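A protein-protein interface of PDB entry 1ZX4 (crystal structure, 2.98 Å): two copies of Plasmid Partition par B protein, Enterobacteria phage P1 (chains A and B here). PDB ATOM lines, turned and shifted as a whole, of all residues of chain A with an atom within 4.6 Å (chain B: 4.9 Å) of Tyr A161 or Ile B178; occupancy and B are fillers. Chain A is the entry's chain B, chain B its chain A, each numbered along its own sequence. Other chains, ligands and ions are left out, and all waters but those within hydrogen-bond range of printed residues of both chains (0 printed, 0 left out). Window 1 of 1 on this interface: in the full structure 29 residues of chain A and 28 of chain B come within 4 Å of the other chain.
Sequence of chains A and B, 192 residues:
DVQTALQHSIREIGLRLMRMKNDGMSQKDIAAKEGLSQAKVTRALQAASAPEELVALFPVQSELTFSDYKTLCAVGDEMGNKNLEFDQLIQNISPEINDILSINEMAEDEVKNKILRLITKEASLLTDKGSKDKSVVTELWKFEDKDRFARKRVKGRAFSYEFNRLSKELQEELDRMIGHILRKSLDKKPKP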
ATOM      1  N   LEU A 140      23.687  14.517  18.313  1.00  0.00           N
ATOM      2  CA  LEU A 140      22.962  13.275  18.080  1.00  0.00           C
ATOM      3  C   LEU A 140      23.544  12.526  16.902  1.00  0.00           C
ATOM      4  O   LEU A 140      23.391  11.309  16.785  1.00  0.00           O
ATOM      5  CB  LEU A 140      21.490  13.578  17.814  1.00  0.00           C
ATOM      6  CG  LEU A 140      20.453  12.754  18.563  1.00  0.00           C
ATOM      7  CD1 LEU A 140      19.074  13.245  18.183  1.00  0.00           C
ATOM      8  CD2 LEU A 140      20.616  11.283  18.217  1.00  0.00           C
ATOM      9  N   ARG A 151      20.577  16.987  16.322  1.00  0.00           N
ATOM     10  CA  ARG A 151      21.023  17.029  17.718  1.00  0.00           C
ATOM     11  C   ARG A 151      19.973  16.967  18.816  1.00  0.00           C
ATOM     12  O   ARG A 151      18.778  16.861  18.555  1.00  0.00           O
ATOM     13  CB  ARG A 151      21.905  18.250  17.967  1.00  0.00           C
ATOM     14  CG  ARG A 151      21.441  19.544  17.357  1.00  0.00           C
ATOM     15  CD  ARG A 151      22.595  20.533  17.481  1.00  0.00           C
ATOM     16  NE  ARG A 151      22.511  21.678  16.577  1.00  0.00           N
ATOM     17  CZ  ARG A 151      21.511  22.554  16.575  1.00  0.00           C
ATOM     18  NH1 ARG A 151      20.504  22.402  17.430  1.00  0.00           N
ATOM     19  NH2 ARG A 151      21.531  23.593  15.741  1.00  0.00           N
ATOM     20  N   LYS A 152      20.447  17.026  20.058  1.00  0.00           N
ATOM     21  CA  LYS A 152      19.582  16.977  21.228  1.00  0.00           C
ATOM     22  C   LYS A 152      19.973  18.148  22.094  1.00  0.00           C
ATOM     23  O   LYS A 152      21.168  18.446  22.243  1.00  0.00           O
ATOM     24  CB  LYS A 152      19.797  15.672  21.996  1.00  0.00           C
ATOM     25  CG  LYS A 152      18.585  15.198  22.776  1.00  0.00           C
ATOM     26  CD  LYS A 152      18.403  15.966  24.050  1.00  0.00           C
ATOM     27  CE  LYS A 152      18.689  15.064  25.244  1.00  0.00           C
ATOM     28  NZ  LYS A 152      17.758  13.899  25.344  1.00  0.00           N
ATOM     29  N   PHE A 159      13.601  19.744  26.991  1.00  0.00           N
ATOM     30  CA  PHE A 159      14.489  19.114  26.018  1.00  0.00           C
ATOM     31  C   PHE A 159      13.855  19.177  24.648  1.00  0.00           C
ATOM     32  O   PHE A 159      12.623  19.265  24.522  1.00  0.00           O
ATOM     33  CB  PHE A 159      14.725  17.636  26.366  1.00  0.00           C
ATOM     34  CG  PHE A 159      13.450  16.818  26.483  1.00  0.00           C
ATOM     35  CD1 PHE A 159      12.629  16.934  27.600  1.00  0.00           C
ATOM     36  CD2 PHE A 159      13.064  15.965  25.463  1.00  0.00           C
ATOM     37  CE1 PHE A 159      11.425  16.213  27.701  1.00  0.00           C
ATOM     38  CE2 PHE A 159      11.876  15.248  25.547  1.00  0.00           C
ATOM     39  CZ  PHE A 159      11.047  15.374  26.678  1.00  0.00           C
ATOM     40  N   SER A 160      14.697  19.111  23.622  1.00  0.00           N
ATOM     41  CA  SER A 160      14.198  19.129  22.263  1.00  0.00           C
ATOM     42  C   SER A 160      15.164  18.441  21.312  1.00  0.00           C
ATOM     43  O   SER A 160      16.380  18.450  21.523  1.00  0.00           O
ATOM     44  CB  SER A 160      13.989  20.566  21.812  1.00  0.00           C
ATOM     45  OG  SER A 160      15.216  21.264  21.872  1.00  0.00           O
ATOM     46  N   TYR A 161      14.619  17.842  20.260  1.00  0.00           N
ATOM     47  CA  TYR A 161      15.444  17.191  19.255  1.00  0.00           C
ATOM     48  C   TYR A 161      15.446  18.043  17.989  1.00  0.00           C
ATOM     49  O   TYR A 161      14.539  17.960  17.165  1.00  0.00           O
ATOM     50  CB  TYR A 161      14.891  15.813  18.980  1.00  0.00           C
ATOM     51  CG  TYR A 161      14.703  15.066  20.250  1.00  0.00           C
ATOM     52  CD1 TYR A 161      15.735  14.311  20.803  1.00  0.00           C
ATOM     53  CD2 TYR A 161      13.513  15.154  20.931  1.00  0.00           C
ATOM     54  CE1 TYR A 161      15.576  13.661  22.014  1.00  0.00           C
ATOM     55  CE2 TYR A 161      13.338  14.511  22.139  1.00  0.00           C
ATOM     56  CZ  TYR A 161      14.363  13.771  22.676  1.00  0.00           C
ATOM     57  OH  TYR A 161      14.125  13.158  23.879  1.00  0.00           O
ATOM     58  N   GLU A 162      16.475  18.871  17.869  1.00  0.00           N
ATOM     59  CA  GLU A 162      16.654  19.775  16.748  1.00  0.00           C
ATOM     60  C   GLU A 162      17.356  19.150  15.556  1.00  0.00           C
ATOM     61  O   GLU A 162      18.434  18.592  15.680  1.00  0.00           O
ATOM     62  CB  GLU A 162      17.463  20.978  17.212  1.00  0.00           C
ATOM     63  CG  GLU A 162      16.672  21.965  18.058  1.00  0.00           C
ATOM     64  CD  GLU A 162      17.509  22.661  19.129  1.00  0.00           C
ATOM     65  OE1 GLU A 162      18.732  22.851  18.929  1.00  0.00           O
ATOM     66  OE2 GLU A 162      16.928  23.032  20.174  1.00  0.00           O
ATOM     67  N   PHE A 163      16.747  19.259  14.391  1.00  0.00           N
ATOM     68  CA  PHE A 163      17.346  18.727  13.176  1.00  0.00           C
ATOM     69  C   PHE A 163      17.333  19.821  12.113  1.00  0.00           C
ATOM     70  O   PHE A 163      16.767  20.908  12.307  1.00  0.00           O
ATOM     71  CB  PHE A 163      16.548  17.554  12.650  1.00  0.00           C
ATOM     72  CG  PHE A 163      16.216  16.546  13.679  1.00  0.00           C
ATOM     73  CD1 PHE A 163      17.185  15.708  14.177  1.00  0.00           C
ATOM     74  CD2 PHE A 163      14.912  16.402  14.120  1.00  0.00           C
ATOM     75  CE1 PHE A 163      16.856  14.732  15.108  1.00  0.00           C
ATOM     76  CE2 PHE A 163      14.577  15.437  15.047  1.00  0.00           C
ATOM     77  CZ  PHE A 163      15.548  14.595  15.540  1.00  0.00           C
ATOM     78  N   PHE B 159      13.963  21.859  11.289  1.00  0.00           N
ATOM     79  CA  PHE B 159      12.767  21.561  12.075  1.00  0.00           C
ATOM     80  C   PHE B 159      13.182  20.899  13.368  1.00  0.00           C
ATOM     81  O   PHE B 159      14.132  20.121  13.373  1.00  0.00           O
ATOM     82  CB  PHE B 159      11.869  20.598  11.311  1.00  0.00           C
ATOM     83  CG  PHE B 159      12.473  19.228  11.121  1.00  0.00           C
ATOM     84  CD1 PHE B 159      13.670  19.068  10.419  1.00  0.00           C
ATOM     85  CD2 PHE B 159      11.836  18.095  11.629  1.00  0.00           C
ATOM     86  CE1 PHE B 159      14.221  17.800  10.223  1.00  0.00           C
ATOM     87  CE2 PHE B 159      12.374  16.825  11.442  1.00  0.00           C
ATOM     88  CZ  PHE B 159      13.569  16.674  10.737  1.00  0.00           C
ATOM     89  N   SER B 160      12.465  21.178  14.455  1.00  0.00           N
ATOM     90  CA  SER B 160      12.803  20.587  15.746  1.00  0.00           C
ATOM     91  C   SER B 160      11.605  20.158  16.574  1.00  0.00           C
ATOM     92  O   SER B 160      10.480  20.622  16.370  1.00  0.00           O
ATOM     93  CB  SER B 160      13.597  21.574  16.558  1.00  0.00           C
ATOM     94  OG  SER B 160      12.739  22.638  16.872  1.00  0.00           O
ATOM     95  N   TYR B 161      11.860  19.275  17.529  1.00  0.00           N
ATOM     96  CA  TYR B 161      10.811  18.794  18.395  1.00  0.00           C
ATOM     97  C   TYR B 161      11.118  19.287  19.784  1.00  0.00           C
ATOM     98  O   TYR B 161      12.076  18.851  20.403  1.00  0.00           O
ATOM     99  CB  TYR B 161      10.778  17.288  18.324  1.00  0.00           C
ATOM    100  CG  TYR B 161      10.377  16.832  16.952  1.00  0.00           C
ATOM    101  CD1 TYR B 161       9.039  16.850  16.557  1.00  0.00           C
ATOM    102  CD2 TYR B 161      11.333  16.427  16.031  1.00  0.00           C
ATOM    103  CE1 TYR B 161       8.661  16.472  15.273  1.00  0.00           C
ATOM    104  CE2 TYR B 161      10.972  16.047  14.745  1.00  0.00           C
ATOM    105  CZ  TYR B 161       9.628  16.072  14.370  1.00  0.00           C
ATOM    106  OH  TYR B 161       9.248  15.694  13.101  1.00  0.00           O
ATOM    107  N   PHE B 163      10.004  20.030  23.784  1.00  0.00           N
ATOM    108  CA  PHE B 163       9.197  19.546  24.900  1.00  0.00           C
ATOM    109  C   PHE B 163       9.630  20.213  26.191  1.00  0.00           C
ATOM    110  O   PHE B 163      10.816  20.520  26.384  1.00  0.00           O
ATOM    111  CB  PHE B 163       9.398  18.048  25.046  1.00  0.00           C
ATOM    112  CG  PHE B 163       9.127  17.247  23.786  1.00  0.00           C
ATOM    113  CD1 PHE B 163       7.837  16.838  23.463  1.00  0.00           C
ATOM    114  CD2 PHE B 163      10.181  16.805  22.983  1.00  0.00           C
ATOM    115  CE1 PHE B 163       7.615  15.976  22.360  1.00  0.00           C
ATOM    116  CE2 PHE B 163       9.963  15.962  21.895  1.00  0.00           C
ATOM    117  CZ  PHE B 163       8.695  15.543  21.582  1.00  0.00           C
ATOM    118  N   LEU B 170       9.521   9.731  28.887  1.00  0.00           N
ATOM    119  CA  LEU B 170       9.526  10.254  27.537  1.00  0.00           C
ATOM    120  C   LEU B 170      10.889  10.597  26.971  1.00  0.00           C
ATOM    121  O   LEU B 170      11.211  10.151  25.888  1.00  0.00           O
ATOM    122  CB  LEU B 170       8.587  11.436  27.432  1.00  0.00           C
ATOM    123  CG  LEU B 170       7.161  10.984  27.169  1.00  0.00           C
ATOM    124  CD1 LEU B 170       6.358  12.148  26.672  1.00  0.00           C
ATOM    125  CD2 LEU B 170       7.177   9.926  26.105  1.00  0.00           C
ATOM    126  N   GLN B 171      11.706  11.374  27.662  1.00  0.00           N
ATOM    127  CA  GLN B 171      13.018  11.656  27.081  1.00  0.00           C
ATOM    128  C   GLN B 171      13.657  10.312  26.815  1.00  0.00           C
ATOM    129  O   GLN B 171      14.390  10.126  25.849  1.00  0.00           O
ATOM    130  CB  GLN B 171      13.910  12.408  28.050  1.00  0.00           C
ATOM    131  CG  GLN B 171      13.549  13.799  28.209  1.00  0.00           C
ATOM    132  CD  GLN B 171      13.828  14.243  29.599  1.00  0.00           C
ATOM    133  OE1 GLN B 171      14.993  14.302  30.013  1.00  0.00           O
ATOM    134  NE2 GLN B 171      12.760  14.545  30.357  1.00  0.00           N
ATOM    135  N   GLU B 173      12.217   7.237  26.151  1.00  0.00           N
ATOM    136  CA  GLU B 173      11.678   6.672  24.927  1.00  0.00           C
ATOM    137  C   GLU B 173      12.162   7.399  23.679  1.00  0.00           C
ATOM    138  O   GLU B 173      12.830   6.815  22.820  1.00  0.00           O
ATOM    139  CB  GLU B 173      10.141   6.679  24.995  1.00  0.00           C
ATOM    140  CG  GLU B 173       9.566   5.516  25.808  1.00  0.00           C
ATOM    141  CD  GLU B 173       8.104   5.195  25.490  1.00  0.00           C
ATOM    142  OE1 GLU B 173       7.762   5.076  24.297  1.00  0.00           O
ATOM    143  OE2 GLU B 173       7.289   5.039  26.429  1.00  0.00           O
ATOM    144  N   LEU B 174      11.811   8.676  23.572  1.00  0.00           N
ATOM    145  CA  LEU B 174      12.215   9.477  22.424  1.00  0.00           C
ATOM    146  C   LEU B 174      13.697   9.267  22.157  1.00  0.00           C
ATOM    147  O   LEU B 174      14.065   8.681  21.147  1.00  0.00           O
ATOM    148  CB  LEU B 174      11.926  10.959  22.674  1.00  0.00           C
ATOM    149  CG  LEU B 174      10.453  11.278  22.987  1.00  0.00           C
ATOM    150  CD1 LEU B 174      10.273  12.785  23.152  1.00  0.00           C
ATOM    151  CD2 LEU B 174       9.553  10.764  21.890  1.00  0.00           C
ATOM    152  N   ASP B 175      14.549   9.729  23.060  1.00  0.00           N
ATOM    153  CA  ASP B 175      15.990   9.562  22.885  1.00  0.00           C
ATOM    154  C   ASP B 175      16.350   8.228  22.232  1.00  0.00           C
ATOM    155  O   ASP B 175      17.161   8.165  21.304  1.00  0.00           O
ATOM    156  CB  ASP B 175      16.708   9.649  24.236  1.00  0.00           C
ATOM    157  CG  ASP B 175      17.081  11.077  24.617  1.00  0.00           C
ATOM    158  OD1 ASP B 175      16.238  11.798  25.197  1.00  0.00           O
ATOM    159  OD2 ASP B 175      18.229  11.484  24.328  1.00  0.00           O
ATOM    160  N   ARG B 176      15.733   7.166  22.737  1.00  0.00           N
ATOM    161  CA  ARG B 176      15.964   5.803  22.274  1.00  0.00           C
ATOM    162  C   ARG B 176      15.556   5.642  20.831  1.00  0.00           C
ATOM    163  O   ARG B 176      16.381   5.322  19.986  1.00  0.00           O
ATOM    164  CB  ARG B 176      15.162   4.833  23.139  1.00  0.00           C
ATOM    165  CG  ARG B 176      15.575   3.392  23.047  1.00  0.00           C
ATOM    166  CD  ARG B 176      14.601   2.527  23.802  1.00  0.00           C
ATOM    167  NE  ARG B 176      14.410   3.000  25.175  1.00  0.00           N
ATOM    168  CZ  ARG B 176      15.406   3.306  26.002  1.00  0.00           C
ATOM    169  NH1 ARG B 176      16.668   3.201  25.592  1.00  0.00           N
ATOM    170  NH2 ARG B 176      15.150   3.683  27.247  1.00  0.00           N
ATOM    171  N   MET B 177      14.275   5.856  20.559  1.00  0.00           N
ATOM    172  CA  MET B 177      13.732   5.739  19.209  1.00  0.00           C
ATOM    173  C   MET B 177      14.332   6.757  18.211  1.00  0.00           C
ATOM    174  O   MET B 177      14.593   6.416  17.060  1.00  0.00           O
ATOM    175  CB  MET B 177      12.197   5.848  19.273  1.00  0.00           C
ATOM    176  CG  MET B 177      11.455   5.826  17.954  1.00  0.00           C
ATOM    177  SD  MET B 177      11.798   7.448  16.995  1.00  0.00           S
ATOM    178  CE  MET B 177      11.053   8.726  18.230  1.00  0.00           C
ATOM    179  N   ILE B 178      14.553   8.000  18.612  1.00  0.00           N
ATOM    180  CA  ILE B 178      15.140   8.937  17.668  1.00  0.00           C
ATOM    181  C   ILE B 178      16.516   8.420  17.236  1.00  0.00           C
ATOM    182  O   ILE B 178      16.841   8.362  16.052  1.00  0.00           O
ATOM    183  CB  ILE B 178      15.290  10.359  18.290  1.00  0.00           C
ATOM    184  CG1 ILE B 178      13.948  11.078  18.254  1.00  0.00           C
ATOM    185  CG2 ILE B 178      16.339  11.196  17.540  1.00  0.00           C
ATOM    186  CD1 ILE B 178      13.963  12.367  19.054  1.00  0.00           C
ATOM    187  N   GLY B 179      17.320   8.019  18.203  1.00  0.00           N
ATOM    188  CA  GLY B 179      18.654   7.552  17.882  1.00  0.00           C
ATOM    189  C   GLY B 179      18.713   6.312  17.021  1.00  0.00           C
ATOM    190  O   GLY B 179      19.671   6.099  16.280  1.00  0.00           O
ATOM    191  N   HIS B 180      17.695   5.481  17.111  1.00  0.00           N
ATOM    192  CA  HIS B 180      17.698   4.269  16.330  1.00  0.00           C
ATOM    193  C   HIS B 180      17.105   4.498  14.942  1.00  0.00           C
ATOM    194  O   HIS B 180      17.413   3.784  13.992  1.00  0.00           O
ATOM    195  CB  HIS B 180      16.960   3.194  17.110  1.00  0.00           C
ATOM    196  CG  HIS B 180      16.384   2.115  16.264  1.00  0.00           C
ATOM    197  ND1 HIS B 180      15.174   2.254  15.619  1.00  0.00           N
ATOM    198  CD2 HIS B 180      16.820   0.863  15.988  1.00  0.00           C
ATOM    199  CE1 HIS B 180      14.885   1.130  14.988  1.00  0.00           C
ATOM    200  NE2 HIS B 180      15.866   0.270  15.196  1.00  0.00           N
ATOM    201  N   ILE B 181      16.260   5.512  14.823  1.00  0.00           N
ATOM    202  CA  ILE B 181      15.662   5.847  13.536  1.00  0.00           C
ATOM    203  C   ILE B 181      16.765   6.525  12.738  1.00  0.00           C
ATOM    204  O   ILE B 181      16.833   6.390  11.523  1.00  0.00           O
ATOM    205  CB  ILE B 181      14.459   6.810  13.706  1.00  0.00           C
ATOM    206  CG1 ILE B 181      13.250   6.033  14.245  1.00  0.00           C
ATOM    207  CG2 ILE B 181      14.148   7.507  12.394  1.00  0.00           C
ATOM    208  CD1 ILE B 181      12.855   4.818  13.417  1.00  0.00           C
ATOM    209  N   LEU B 182      17.627   7.260  13.435  1.00  0.00           N
ATOM    210  CA  LEU B 182      18.744   7.921  12.788  1.00  0.00           C
ATOM    211  C   LEU B 182      19.778   6.869  12.430  1.00  0.00           C
ATOM    212  O   LEU B 182      20.748   7.143  11.743  1.00  0.00           O
ATOM    213  CB  LEU B 182      19.370   8.975  13.703  1.00  0.00           C
ATOM    214  CG  LEU B 182      18.589  10.279  13.822  1.00  0.00           C
ATOM    215  CD1 LEU B 182      19.551  11.437  14.075  1.00  0.00           C
ATOM    216  CD2 LEU B 182      17.822  10.522  12.523  1.00  0.00           C
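Phe A159 touches Phe B163, and with the chains exchanged Phe A163 touches Phe B159. Ser A160 touches Tyr B161, and with the chains exchanged Tyr A161 touches Ser B160. Tyr B161 touches its own counterpart, Tyr A161. Tyr A161 touches Phe B163, and with the chains exchanged Phe A163 touches Tyr B161. Positions printed for both chains: 159, 160, 161 and 163. Of the 16 pairs that touch across the chains among the printed residues, 7 have their exchanged pair printed and touching as well.
Hydrophobic or aromatic side chains of chain B within 4 Å of the printed part of chain A: Phe B159, Tyr B161, Phe B163, Leu B174 and Ile B178. Of the 8 printed residues of chain A, 7 touch a printed residue of chain B. Hydrophobic or aromatic side chains of chain A within 4 Å of the printed part of chain B: Leu A140, Phe A159, Tyr A161 and Phe A163. Among the printed residues, Asp or Glu carboxylates within 4 Å of a Lys or Arg side-chain nitrogen of the other chain: Lys A152 with Asp B175 (2.6 Å).
Among the printed residues, pairs that only touch across the chains: Ser A160 with Tyr B161 (2.8 Å), Tyr A161 with Ile B178 (3.0 Å), Phe A159 with Gln B171 (3.3 Å), Tyr A161 with Leu B174 (3.3 Å), Glu A162 with Ser B160 (3.4 Å), Tyr A161 with Ser B160 (3.5 Å), Leu A140 with Ile B178 (3.5 Å), Phe A163 with Tyr B161 (3.5 Å), Tyr A161 with Gln B171 (3.6 Å), Tyr A161 with Phe B163 (3.7 Å) and Phe A159 with Leu B174 (3.8 Å).
Of chain B, only Ser B160 (3.5 Å), Tyr B161 (2.7 Å), Phe B163 (3.7 Å), Gln B171 (3.6 Å), Leu B174 (3.3 Å), Asp B175 (2.8 Å) and Ile B178 (3.0 Å) come within 4 Å of Tyr A161. Of chain A, only Leu A140 and Tyr A161 come within 4 Å of Ile B178. Of the printed residues of chain A, Phe B159 touches Phe A163 (2.9 Å). Of the printed residues of chain A, Tyr B161 touches Ser A160, Tyr A161 and Phe A163. Of the printed residues of chain B, Leu A140 touches Ile B178 (3.5 Å). Printed residues of chain A within 4 Å of Gln B171: Phe A159 (3.3 Å) and Tyr A161 (3.6 Å). Printed residues of chain B within 4 Å of Glu A162: Ser B160 (3.4 Å). The nearest residue of chain B that does not touch Tyr A161 is Phe B159 (4.4 Å). The nearest printed residue of chain A that does not touch Asp B175 is Phe A159 (5.2 Å).
The backbone carbonyl oxygen of Phe B159 sits at hydrogen-bond distance from the backbone NH of Phe A163, at 2.9 Å. The backbone carbonyl oxygen of Tyr B161 sits at hydrogen-bond distance from the backbone NH of Tyr A161, at 2.7 Å. N of Phe B163 is in hydrogen-bond range of O of Phe A159 (2.8 Å). NZ of Lys A152 is in salt-bridge range of OD1 of Asp B175, at 2.6 Å. OD1 of Asp B175 sits at hydrogen-bond distance from OH of Tyr A161, 2.8 Å away.
The backbone carbonyl oxygen of Gln B171 lies close to the side-chain carboxylate of Asp B175 (2.6 Å). N of Arg A151 lies within hydrogen-bond range of O of Glu A162, at 2.8 Å. The side-chain carboxylate of Glu A162 is in hydrogen-bond range of the side-chain hydroxyl of Ser A160, 3.0 Å away.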
